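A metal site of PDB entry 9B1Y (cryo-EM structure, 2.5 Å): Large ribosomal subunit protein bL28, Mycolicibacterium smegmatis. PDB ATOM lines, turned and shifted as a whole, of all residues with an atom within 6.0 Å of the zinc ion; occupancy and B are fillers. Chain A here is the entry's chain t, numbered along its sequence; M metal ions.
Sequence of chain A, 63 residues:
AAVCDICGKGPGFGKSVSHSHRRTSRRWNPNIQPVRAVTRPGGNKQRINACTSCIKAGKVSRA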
ATOM      1  N   CYS A   4     -11.729  32.643  -4.147  1.00  0.00           N
ATOM      2  CA  CYS A   4     -11.255  31.317  -4.508  1.00  0.00           C
ATOM      3  C   CYS A   4      -9.933  31.453  -5.245  1.00  0.00           C
ATOM      4  O   CYS A   4      -9.763  32.355  -6.068  1.00  0.00           O
ATOM      5  CB  CYS A   4     -12.275  30.573  -5.358  1.00  0.00           C
ATOM      6  SG  CYS A   4     -12.080  28.788  -5.240  1.00  0.00           S
ATOM      7  N   ASP A   5      -9.008  30.537  -4.952  1.00  0.00           N
ATOM      8  CA  ASP A   5      -7.627  30.754  -5.372  1.00  0.00           C
ATOM      9  C   ASP A   5      -7.495  30.858  -6.881  1.00  0.00           C
ATOM     10  O   ASP A   5      -6.852  31.794  -7.384  1.00  0.00           O
ATOM     11  CB  ASP A   5      -6.743  29.630  -4.835  1.00  0.00           C
ATOM     12  CG  ASP A   5      -6.267  29.891  -3.427  1.00  0.00           C
ATOM     13  OD1 ASP A   5      -5.387  30.752  -3.261  1.00  0.00           O
ATOM     14  OD2 ASP A   5      -6.775  29.234  -2.494  1.00  0.00           O
ATOM     15  N   ILE A   6      -8.090  29.938  -7.634  1.00  0.00           N
ATOM     16  CA  ILE A   6      -7.843  29.818  -9.060  1.00  0.00           C
ATOM     17  C   ILE A   6      -8.935  30.465  -9.887  1.00  0.00           C
ATOM     18  O   ILE A   6      -8.659  31.213 -10.825  1.00  0.00           O
ATOM     19  CB  ILE A   6      -7.651  28.338  -9.450  1.00  0.00           C
ATOM     20  CG1 ILE A   6      -8.943  27.569  -9.212  1.00  0.00           C
ATOM     21  CG2 ILE A   6      -6.539  27.722  -8.643  1.00  0.00           C
ATOM     22  CD1 ILE A   6      -8.752  26.097  -9.090  1.00  0.00           C
ATOM     23  N   CYS A   7     -10.195  30.175  -9.574  1.00  0.00           N
ATOM     24  CA  CYS A   7     -11.326  30.700 -10.318  1.00  0.00           C
ATOM     25  C   CYS A   7     -11.487  32.210 -10.202  1.00  0.00           C
ATOM     26  O   CYS A   7     -12.171  32.811 -11.047  1.00  0.00           O
ATOM     27  CB  CYS A   7     -12.606  30.025  -9.834  1.00  0.00           C
ATOM     28  SG  CYS A   7     -13.260  30.787  -8.350  1.00  0.00           S
ATOM     29  N   GLY A   8     -10.879  32.845  -9.211  1.00  0.00           N
ATOM     30  CA  GLY A   8     -10.981  34.289  -9.064  1.00  0.00           C
ATOM     31  C   GLY A   8     -12.399  34.773  -8.874  1.00  0.00           C
ATOM     32  O   GLY A   8     -12.845  35.691  -9.569  1.00  0.00           O
ATOM     33  N   LYS A   9     -13.120  34.151  -7.955  1.00  0.00           N
ATOM     34  CA  LYS A   9     -14.551  34.371  -7.785  1.00  0.00           C
ATOM     35  C   LYS A   9     -14.808  35.165  -6.504  1.00  0.00           C
ATOM     36  O   LYS A   9     -15.091  34.581  -5.454  1.00  0.00           O
ATOM     37  CB  LYS A   9     -15.271  33.029  -7.746  1.00  0.00           C
ATOM     38  CG  LYS A   9     -15.839  32.583  -9.073  1.00  0.00           C
ATOM     39  CD  LYS A   9     -16.302  31.145  -8.966  1.00  0.00           C
ATOM     40  CE  LYS A   9     -17.583  31.018  -8.204  1.00  0.00           C
ATOM     41  NZ  LYS A   9     -18.701  31.658  -8.907  1.00  0.00           N
ATOM     42  N   ASN A  49      -7.492  27.519  -0.751  1.00  0.00           N
ATOM     43  CA  ASN A  49      -8.903  27.864  -0.695  1.00  0.00           C
ATOM     44  C   ASN A  49      -9.523  27.608  -2.063  1.00  0.00           C
ATOM     45  O   ASN A  49      -9.186  28.296  -3.032  1.00  0.00           O
ATOM     46  CB  ASN A  49      -9.082  29.320  -0.281  1.00  0.00           C
ATOM     47  CG  ASN A  49      -9.396  29.470   1.196  1.00  0.00           C
ATOM     48  OD1 ASN A  49      -9.016  28.626   2.011  1.00  0.00           O
ATOM     49  ND2 ASN A  49     -10.076  30.551   1.551  1.00  0.00           N
ATOM     50  N   ALA A  50     -10.407  26.623  -2.156  1.00  0.00           N
ATOM     51  CA  ALA A  50     -11.017  26.235  -3.421  1.00  0.00           C
ATOM     52  C   ALA A  50     -12.525  26.227  -3.280  1.00  0.00           C
ATOM     53  O   ALA A  50     -13.049  25.874  -2.209  1.00  0.00           O
ATOM     54  CB  ALA A  50     -10.522  24.870  -3.881  1.00  0.00           C
ATOM     55  N   CYS A  51     -13.223  26.609  -4.340  1.00  0.00           N
ATOM     56  CA  CYS A  51     -14.675  26.565  -4.316  1.00  0.00           C
ATOM     57  C   CYS A  51     -15.169  25.270  -4.966  1.00  0.00           C
ATOM     58  O   CYS A  51     -14.405  24.510  -5.555  1.00  0.00           O
ATOM     59  CB  CYS A  51     -15.291  27.757  -5.056  1.00  0.00           C
ATOM     60  SG  CYS A  51     -15.109  27.695  -6.856  1.00  0.00           S
ATOM     61  N   THR A  52     -16.472  25.043  -4.865  1.00  0.00           N
ATOM     62  CA  THR A  52     -17.044  23.851  -5.480  1.00  0.00           C
ATOM     63  C   THR A  52     -16.865  23.867  -6.987  1.00  0.00           C
ATOM     64  O   THR A  52     -16.609  22.821  -7.593  1.00  0.00           O
ATOM     65  CB  THR A  52     -18.519  23.719  -5.127  1.00  0.00           C
ATOM     66  OG1 THR A  52     -18.691  23.886  -3.715  1.00  0.00           O
ATOM     67  CG2 THR A  52     -19.041  22.363  -5.544  1.00  0.00           C
ATOM     68  N   SER A  53     -17.023  25.032  -7.619  1.00  0.00           N
ATOM     69  CA  SER A  53     -16.843  25.108  -9.062  1.00  0.00           C
ATOM     70  C   SER A  53     -15.434  24.672  -9.436  1.00  0.00           C
ATOM     71  O   SER A  53     -15.243  23.893 -10.365  1.00  0.00           O
ATOM     72  CB  SER A  53     -17.127  26.513  -9.570  1.00  0.00           C
ATOM     73  OG  SER A  53     -17.151  26.541 -10.982  1.00  0.00           O
ATOM     74  N   CYS A  54     -14.430  25.168  -8.717  1.00  0.00           N
ATOM     75  CA  CYS A  54     -13.061  24.750  -9.001  1.00  0.00           C
ATOM     76  C   CYS A  54     -12.875  23.262  -8.748  1.00  0.00           C
ATOM     77  O   CYS A  54     -12.261  22.557  -9.565  1.00  0.00           O
ATOM     78  CB  CYS A  54     -12.081  25.569  -8.180  1.00  0.00           C
ATOM     79  SG  CYS A  54     -11.939  27.264  -8.745  1.00  0.00           S
ATOM     80  N   ILE A  55     -13.406  22.761  -7.643  1.00  0.00           N
ATOM     81  CA  ILE A  55     -13.234  21.349  -7.331  1.00  0.00           C
ATOM     82  C   ILE A  55     -13.759  20.495  -8.472  1.00  0.00           C
ATOM     83  O   ILE A  55     -13.063  19.612  -8.980  1.00  0.00           O
ATOM     84  CB  ILE A  55     -13.911  20.998  -5.997  1.00  0.00           C
ATOM     85  CG1 ILE A  55     -13.162  21.637  -4.841  1.00  0.00           C
ATOM     86  CG2 ILE A  55     -13.969  19.496  -5.818  1.00  0.00           C
ATOM     87  CD1 ILE A  55     -11.693  21.832  -5.119  1.00  0.00           C
HETATM   88 ZN    ZN M   1     -13.082  28.703  -7.321  1.00  0.00          ZN
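The backbone NH of Ser 53 sits close to the side-chain sulfur of Cys 51. SG of Cys 4 sits close to O of Asn 49. N of Lys 9 lies close to SG of Cys 7.
The zinc ion is bound by SG of Cys 51 (2.3 Å). The zinc ion is bound by SG of Cys 4, 2.3 Å away. SG of Cys 54 is bound to the zinc ion (2.3 Å). The side-chain sulfur (SG) of Cys 7 is bound to the zinc ion, at 2.3 Å.
Along chain A the residues within 4 Å of the zinc ion span positions 4 to 54.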
